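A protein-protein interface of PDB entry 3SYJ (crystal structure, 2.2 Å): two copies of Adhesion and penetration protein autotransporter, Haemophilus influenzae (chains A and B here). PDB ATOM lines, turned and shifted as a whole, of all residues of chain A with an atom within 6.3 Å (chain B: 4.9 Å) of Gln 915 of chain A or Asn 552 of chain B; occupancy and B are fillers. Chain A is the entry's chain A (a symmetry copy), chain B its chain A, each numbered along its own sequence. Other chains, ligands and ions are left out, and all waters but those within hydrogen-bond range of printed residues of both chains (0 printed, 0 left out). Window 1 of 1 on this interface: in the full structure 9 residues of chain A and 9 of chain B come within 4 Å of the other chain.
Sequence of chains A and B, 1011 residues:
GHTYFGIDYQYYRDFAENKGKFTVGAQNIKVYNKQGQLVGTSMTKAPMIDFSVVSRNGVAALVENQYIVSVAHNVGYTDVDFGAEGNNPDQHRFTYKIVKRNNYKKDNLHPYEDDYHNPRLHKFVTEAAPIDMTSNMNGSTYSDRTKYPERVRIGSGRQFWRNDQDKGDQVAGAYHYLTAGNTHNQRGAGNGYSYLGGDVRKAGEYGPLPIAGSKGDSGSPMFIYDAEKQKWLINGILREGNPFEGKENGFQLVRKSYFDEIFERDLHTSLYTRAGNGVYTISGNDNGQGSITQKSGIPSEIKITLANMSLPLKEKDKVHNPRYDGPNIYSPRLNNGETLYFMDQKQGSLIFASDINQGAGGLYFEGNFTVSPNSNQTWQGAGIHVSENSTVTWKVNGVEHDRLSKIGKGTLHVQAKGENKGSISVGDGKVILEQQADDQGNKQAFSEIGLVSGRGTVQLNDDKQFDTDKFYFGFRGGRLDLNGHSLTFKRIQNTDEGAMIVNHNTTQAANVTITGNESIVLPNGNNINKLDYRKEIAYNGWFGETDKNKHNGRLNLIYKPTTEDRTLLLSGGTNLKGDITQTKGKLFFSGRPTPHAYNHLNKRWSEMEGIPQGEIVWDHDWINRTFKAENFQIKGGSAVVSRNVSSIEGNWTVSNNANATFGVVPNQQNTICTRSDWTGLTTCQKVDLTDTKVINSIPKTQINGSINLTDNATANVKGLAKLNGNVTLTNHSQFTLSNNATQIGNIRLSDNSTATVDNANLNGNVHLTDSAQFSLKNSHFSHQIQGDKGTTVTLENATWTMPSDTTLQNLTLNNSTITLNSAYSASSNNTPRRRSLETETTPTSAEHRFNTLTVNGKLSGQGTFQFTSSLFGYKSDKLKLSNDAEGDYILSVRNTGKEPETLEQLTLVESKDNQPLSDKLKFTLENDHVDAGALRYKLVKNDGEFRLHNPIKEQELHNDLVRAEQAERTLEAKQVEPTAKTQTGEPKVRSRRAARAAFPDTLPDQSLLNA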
ATOM      1  N   ASN A 883      22.170  -2.803  -4.327  1.00  0.00           N
ATOM      2  CA  ASN A 883      21.394  -2.384  -3.169  1.00  0.00           C
ATOM      3  C   ASN A 883      20.126  -1.636  -3.556  1.00  0.00           C
ATOM      4  O   ASN A 883      19.163  -1.597  -2.791  1.00  0.00           O
ATOM      5  CB  ASN A 883      22.245  -1.525  -2.236  1.00  0.00           C
ATOM      6  CG  ASN A 883      23.011  -2.354  -1.222  1.00  0.00           C
ATOM      7  OD1 ASN A 883      24.199  -2.128  -0.984  1.00  0.00           O
ATOM      8  ND2 ASN A 883      22.330  -3.329  -0.620  1.00  0.00           N
ATOM      9  N   SER A 911      23.684 -10.451  -4.878  1.00  0.00           N
ATOM     10  CA  SER A 911      24.151  -9.076  -4.882  1.00  0.00           C
ATOM     11  C   SER A 911      25.418  -8.961  -5.720  1.00  0.00           C
ATOM     12  O   SER A 911      26.180  -9.922  -5.843  1.00  0.00           O
ATOM     13  CB  SER A 911      24.424  -8.609  -3.456  1.00  0.00           C
ATOM     14  OG  SER A 911      25.076  -7.354  -3.458  1.00  0.00           O
ATOM     15  N   LYS A 912      25.655  -7.784  -6.272  1.00  0.00           N
ATOM     16  CA  LYS A 912      26.798  -7.543  -7.128  1.00  0.00           C
ATOM     17  C   LYS A 912      28.083  -7.539  -6.328  1.00  0.00           C
ATOM     18  O   LYS A 912      29.139  -7.660  -6.875  1.00  0.00           O
ATOM     19  CB  LYS A 912      26.642  -6.249  -7.948  1.00  0.00           C
ATOM     20  CG  LYS A 912      26.420  -5.016  -7.136  1.00  0.00           C
ATOM     21  CD  LYS A 912      26.300  -3.749  -7.915  1.00  0.00           C
ATOM     22  CE  LYS A 912      27.514  -3.482  -8.730  1.00  0.00           C
ATOM     23  NZ  LYS A 912      27.632  -2.040  -9.058  1.00  0.00           N
ATOM     24  N   ASP A 913      27.961  -7.390  -5.024  1.00  0.00           N
ATOM     25  CA  ASP A 913      29.055  -7.570  -4.095  1.00  0.00           C
ATOM     26  C   ASP A 913      28.458  -8.076  -2.776  1.00  0.00           C
ATOM     27  O   ASP A 913      27.373  -8.589  -2.744  1.00  0.00           O
ATOM     28  CB  ASP A 913      29.651  -6.233  -3.732  1.00  0.00           C
ATOM     29  CG  ASP A 913      28.623  -5.264  -3.294  1.00  0.00           C
ATOM     30  OD1 ASP A 913      28.910  -4.084  -3.245  1.00  0.00           O
ATOM     31  OD2 ASP A 913      27.516  -5.686  -2.995  1.00  0.00           O
ATOM     32  N   ASN A 914      29.203  -7.915  -1.695  1.00  0.00           N
ATOM     33  CA  ASN A 914      28.841  -8.465  -0.405  1.00  0.00           C
ATOM     34  C   ASN A 914      27.679  -7.806   0.323  1.00  0.00           C
ATOM     35  O   ASN A 914      27.162  -8.397   1.218  1.00  0.00           O
ATOM     36  CB  ASN A 914      30.027  -8.523   0.570  1.00  0.00           C
ATOM     37  CG  ASN A 914      31.188  -9.338   0.059  1.00  0.00           C
ATOM     38  OD1 ASN A 914      31.024 -10.427  -0.467  1.00  0.00           O
ATOM     39  ND2 ASN A 914      32.375  -8.808   0.231  1.00  0.00           N
ATOM     40  N   GLN A 915      27.273  -6.602  -0.021  1.00  0.00           N
ATOM     41  CA  GLN A 915      26.092  -6.055   0.632  1.00  0.00           C
ATOM     42  C   GLN A 915      24.833  -6.854   0.313  1.00  0.00           C
ATOM     43  O   GLN A 915      24.689  -7.379  -0.764  1.00  0.00           O
ATOM     44  CB  GLN A 915      25.870  -4.584   0.262  1.00  0.00           C
ATOM     45  CG  GLN A 915      27.110  -3.722   0.254  1.00  0.00           C
ATOM     46  CD  GLN A 915      27.572  -3.256   1.611  1.00  0.00           C
ATOM     47  OE1 GLN A 915      26.821  -3.180   2.547  1.00  0.00           O
ATOM     48  NE2 GLN A 915      28.804  -2.914   1.691  1.00  0.00           N
ATOM     49  N   PRO A 916      23.910  -6.908   1.258  1.00  0.00           N
ATOM     50  CA  PRO A 916      22.666  -7.657   1.129  1.00  0.00           C
ATOM     51  C   PRO A 916      21.595  -6.981   0.275  1.00  0.00           C
ATOM     52  O   PRO A 916      21.553  -5.778   0.185  1.00  0.00           O
ATOM     53  CB  PRO A 916      22.184  -7.744   2.569  1.00  0.00           C
ATOM     54  CG  PRO A 916      23.239  -7.438   3.351  1.00  0.00           C
ATOM     55  CD  PRO A 916      24.172  -6.585   2.652  1.00  0.00           C
ATOM     56  N   LEU A 917      20.737  -7.767  -0.344  1.00  0.00           N
ATOM     57  CA  LEU A 917      19.694  -7.196  -1.189  1.00  0.00           C
ATOM     58  C   LEU A 917      18.614  -6.524  -0.352  1.00  0.00           C
ATOM     59  O   LEU A 917      18.283  -6.989   0.736  1.00  0.00           O
ATOM     60  CB  LEU A 917      19.064  -8.276  -2.070  1.00  0.00           C
ATOM     61  CG  LEU A 917      19.969  -8.928  -3.118  1.00  0.00           C
ATOM     62  CD1 LEU A 917      19.221 -10.032  -3.844  1.00  0.00           C
ATOM     63  CD2 LEU A 917      20.492  -7.894  -4.104  1.00  0.00           C
ATOM     64  N   GLY A 944      21.135 -12.505   2.813  1.00  0.00           N
ATOM     65  CA  GLY A 944      21.060 -11.385   1.889  1.00  0.00           C
ATOM     66  C   GLY A 944      20.825 -11.727   0.427  1.00  0.00           C
ATOM     67  O   GLY A 944      20.803 -10.832  -0.421  1.00  0.00           O
ATOM     68  N   GLU A 945      20.648 -13.012   0.128  1.00  0.00           N
ATOM     69  CA  GLU A 945      20.441 -13.467  -1.246  1.00  0.00           C
ATOM     70  C   GLU A 945      19.267 -14.436  -1.336  1.00  0.00           C
ATOM     71  O   GLU A 945      18.887 -15.049  -0.341  1.00  0.00           O
ATOM     72  CB  GLU A 945      21.709 -14.132  -1.786  1.00  0.00           C
ATOM     73  CG  GLU A 945      22.953 -13.281  -1.621  1.00  0.00           C
ATOM     74  CD  GLU A 945      24.132 -13.785  -2.429  1.00  0.00           C
ATOM     75  OE1 GLU A 945      24.378 -15.011  -2.444  1.00  0.00           O
ATOM     76  OE2 GLU A 945      24.819 -12.945  -3.047  1.00  0.00           O
ATOM     77  N   ASN B 503      26.505   2.593  10.231  1.00  0.00           N
ATOM     78  CA  ASN B 503      25.208   1.961  10.455  1.00  0.00           C
ATOM     79  C   ASN B 503      25.236   0.563   9.876  1.00  0.00           C
ATOM     80  O   ASN B 503      25.132   0.392   8.665  1.00  0.00           O
ATOM     81  CB  ASN B 503      24.073   2.765   9.816  1.00  0.00           C
ATOM     82  CG  ASN B 503      22.718   2.089   9.975  1.00  0.00           C
ATOM     83  OD1 ASN B 503      22.525   1.280  10.881  1.00  0.00           O
ATOM     84  ND2 ASN B 503      21.772   2.427   9.100  1.00  0.00           N
ATOM     85  N   GLY B 544      30.438   6.234   7.622  1.00  0.00           N
ATOM     86  CA  GLY B 544      30.189   5.106   6.748  1.00  0.00           C
ATOM     87  C   GLY B 544      31.216   4.023   6.996  1.00  0.00           C
ATOM     88  O   GLY B 544      32.332   4.298   7.439  1.00  0.00           O
ATOM     89  N   GLU B 545      30.839   2.784   6.716  1.00  0.00           N
ATOM     90  CA  GLU B 545      31.717   1.655   6.950  1.00  0.00           C
ATOM     91  C   GLU B 545      32.652   1.465   5.764  1.00  0.00           C
ATOM     92  O   GLU B 545      32.214   1.464   4.613  1.00  0.00           O
ATOM     93  CB  GLU B 545      30.892   0.391   7.185  1.00  0.00           C
ATOM     94  CG  GLU B 545      31.728  -0.858   7.381  1.00  0.00           C
ATOM     95  CD  GLU B 545      32.641  -0.763   8.589  1.00  0.00           C
ATOM     96  OE1 GLU B 545      32.129  -0.707   9.728  1.00  0.00           O
ATOM     97  OE2 GLU B 545      33.875  -0.744   8.395  1.00  0.00           O
ATOM     98  N   LYS B 550      31.970  -5.920   6.471  1.00  0.00           N
ATOM     99  CA  LYS B 550      30.931  -5.447   7.374  1.00  0.00           C
ATOM    100  C   LYS B 550      29.879  -4.715   6.560  1.00  0.00           C
ATOM    101  O   LYS B 550      30.171  -4.210   5.477  1.00  0.00           O
ATOM    102  CB  LYS B 550      31.519  -4.542   8.456  1.00  0.00           C
ATOM    103  CG  LYS B 550      32.446  -5.285   9.405  1.00  0.00           C
ATOM    104  CD  LYS B 550      32.819  -4.461  10.629  1.00  0.00           C
ATOM    105  CE  LYS B 550      33.637  -5.300  11.610  1.00  0.00           C
ATOM    106  NZ  LYS B 550      33.889  -4.610  12.905  1.00  0.00           N
ATOM    107  N   HIS B 551      28.656  -4.668   7.072  1.00  0.00           N
ATOM    108  CA  HIS B 551      27.560  -4.061   6.329  1.00  0.00           C
ATOM    109  C   HIS B 551      27.582  -2.523   6.355  1.00  0.00           C
ATOM    110  O   HIS B 551      27.570  -1.898   7.418  1.00  0.00           O
ATOM    111  CB  HIS B 551      26.208  -4.617   6.803  1.00  0.00           C
ATOM    112  CG  HIS B 551      25.052  -4.196   5.945  1.00  0.00           C
ATOM    113  ND1 HIS B 551      25.012  -4.423   4.584  1.00  0.00           N
ATOM    114  CD2 HIS B 551      23.895  -3.556   6.251  1.00  0.00           C
ATOM    115  CE1 HIS B 551      23.884  -3.941   4.091  1.00  0.00           C
ATOM    116  NE2 HIS B 551      23.186  -3.416   5.081  1.00  0.00           N
ATOM    117  N   ASN B 552      27.617  -1.917   5.176  1.00  0.00           N
ATOM    118  CA  ASN B 552      27.522  -0.469   5.073  1.00  0.00           C
ATOM    119  C   ASN B 552      26.063  -0.042   4.882  1.00  0.00           C
ATOM    120  O   ASN B 552      25.621   0.210   3.762  1.00  0.00           O
ATOM    121  CB  ASN B 552      28.411   0.050   3.936  1.00  0.00           C
ATOM    122  CG  ASN B 552      28.617   1.556   3.988  1.00  0.00           C
ATOM    123  OD1 ASN B 552      28.498   2.173   5.046  1.00  0.00           O
ATOM    124  ND2 ASN B 552      28.930   2.154   2.841  1.00  0.00           N
ATOM    125  N   GLY B 553      25.321   0.028   5.985  1.00  0.00           N
ATOM    126  CA  GLY B 553      23.912   0.381   5.944  1.00  0.00           C
ATOM    127  C   GLY B 553      23.675   1.844   5.624  1.00  0.00           C
ATOM    128  O   GLY B 553      24.594   2.660   5.725  1.00  0.00           O
ATOM    129  N   ARG B 554      22.449   2.176   5.228  1.00  0.00           N
ATOM    130  CA  ARG B 554      22.131   3.544   4.832  1.00  0.00           C
ATOM    131  C   ARG B 554      22.470   4.499   5.966  1.00  0.00           C
ATOM    132  O   ARG B 554      22.048   4.297   7.101  1.00  0.00           O
ATOM    133  CB  ARG B 554      20.647   3.710   4.469  1.00  0.00           C
ATOM    134  CG  ARG B 554      20.051   2.662   3.539  1.00  0.00           C
ATOM    135  CD  ARG B 554      20.149   3.048   2.065  1.00  0.00           C
ATOM    136  NE  ARG B 554      19.984   4.481   1.840  1.00  0.00           N
ATOM    137  CZ  ARG B 554      20.390   5.098   0.735  1.00  0.00           C
ATOM    138  NH1 ARG B 554      20.976   4.399  -0.229  1.00  0.00           N
ATOM    139  NH2 ARG B 554      20.221   6.407   0.592  1.00  0.00           N
ATOM    140  N   ASN B 575      32.183   7.214   3.376  1.00  0.00           N
ATOM    141  CA  ASN B 575      31.784   6.183   2.432  1.00  0.00           C
ATOM    142  C   ASN B 575      30.295   5.938   2.600  1.00  0.00           C
ATOM    143  O   ASN B 575      29.879   4.866   3.028  1.00  0.00           O
ATOM    144  CB  ASN B 575      32.558   4.891   2.675  1.00  0.00           C
ATOM    145  CG  ASN B 575      32.353   3.883   1.569  1.00  0.00           C
ATOM    146  OD1 ASN B 575      32.339   2.672   1.805  1.00  0.00           O
ATOM    147  ND2 ASN B 575      32.187   4.377   0.349  1.00  0.00           N
ATOM    148  N   LEU B 576      29.493   6.942   2.266  1.00  0.00           N
ATOM    149  CA  LEU B 576      28.088   6.941   2.646  1.00  0.00           C
ATOM    150  C   LEU B 576      27.152   6.335   1.627  1.00  0.00           C
ATOM    151  O   LEU B 576      27.092   6.772   0.481  1.00  0.00           O
ATOM    152  CB  LEU B 576      27.613   8.355   2.959  1.00  0.00           C
ATOM    153  CG  LEU B 576      28.156   8.948   4.252  1.00  0.00           C
ATOM    154  CD1 LEU B 576      27.797  10.416   4.347  1.00  0.00           C
ATOM    155  CD2 LEU B 576      27.619   8.183   5.435  1.00  0.00           C
ATOM    156  N   LYS B 577      26.408   5.330   2.070  1.00  0.00           N
ATOM    157  CA  LYS B 577      25.240   4.877   1.345  1.00  0.00           C
ATOM    158  C   LYS B 577      24.115   5.791   1.818  1.00  0.00           C
ATOM    159  O   LYS B 577      23.364   5.455   2.730  1.00  0.00           O
ATOM    160  CB  LYS B 577      24.941   3.427   1.695  1.00  0.00           C
ATOM    161  CG  LYS B 577      24.799   2.519   0.489  1.00  0.00           C
ATOM    162  CD  LYS B 577      26.164   2.164  -0.097  1.00  0.00           C
ATOM    163  CE  LYS B 577      26.021   1.332  -1.374  1.00  0.00           C
ATOM    164  NZ  LYS B 577      27.251   0.548  -1.687  1.00  0.00           N
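The backbone NH of Asn 552 of chain B sits at hydrogen-bond distance from the side-chain amide oxygen of Gln 915 of chain A (3.0 Å). A ring nitrogen (ND1) of His 551 of chain B is in hydrogen-bond range of the side-chain amide oxygen of Gln 915 of chain A (3.0 Å).
The side-chain amide nitrogen (ND2) of Asn 552 of chain B lies within hydrogen-bond range of the backbone carbonyl oxygen (O) of Asn 575 of chain B, 2.9 Å away. The side-chain amide nitrogen of Asn 883 of chain A lies within hydrogen-bond range of the backbone carbonyl oxygen of Pro 916 of chain A. The side-chain hydroxyl (OG) of Ser 911 of chain A is in hydrogen-bond range of the backbone carbonyl oxygen (O) of Gln 915 of chain A, 2.7 Å away. The side-chain carboxylate (OD2) of Asp 913 of chain A is in hydrogen-bond range of the backbone NH (N) of Gln 915 of chain A (3.1 Å). The backbone NH (N) of Glu 545 of chain B lies within hydrogen-bond range of the side-chain amide oxygen (OD1) of Asn 552 of chain B, at 2.9 Å.
Among the printed residues, merely in contact across the chains: Asn 883 of chain A with Lys 577 of chain B (3.9 Å) and Pro 916 of chain A with His 551 of chain B (3.0 Å).
Of the printed residues of chain B, Asn 883 of chain A touches Lys 577. Gln 915 of chain A touches just these residues of chain B: His 551 (3.0 Å) and Asn 552 (3.0 Å). Printed residues of chain B within 4 Å of Pro 916 of chain A: His 551. Of the printed residues of chain A, Asn 552 of chain B touches Gln 915. The nearest residue of chain A that does not touch Asn 552 of chain B is Asn 883 of chain A (5.5 Å).
Of the 10 printed residues of chain A, 3 touch a printed residue of chain B. Of the 11 printed residues of chain B, 3 touch a printed residue of chain A. Among the printed residues, no Asp or Glu carboxylate lies within 4 Å of a Lys or Arg side-chain nitrogen of the other chain.
No position is printed for both chains. Of the 4 pairs that touch across the chains among the printed residues, none has its exchanged pair printed and touching as well.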
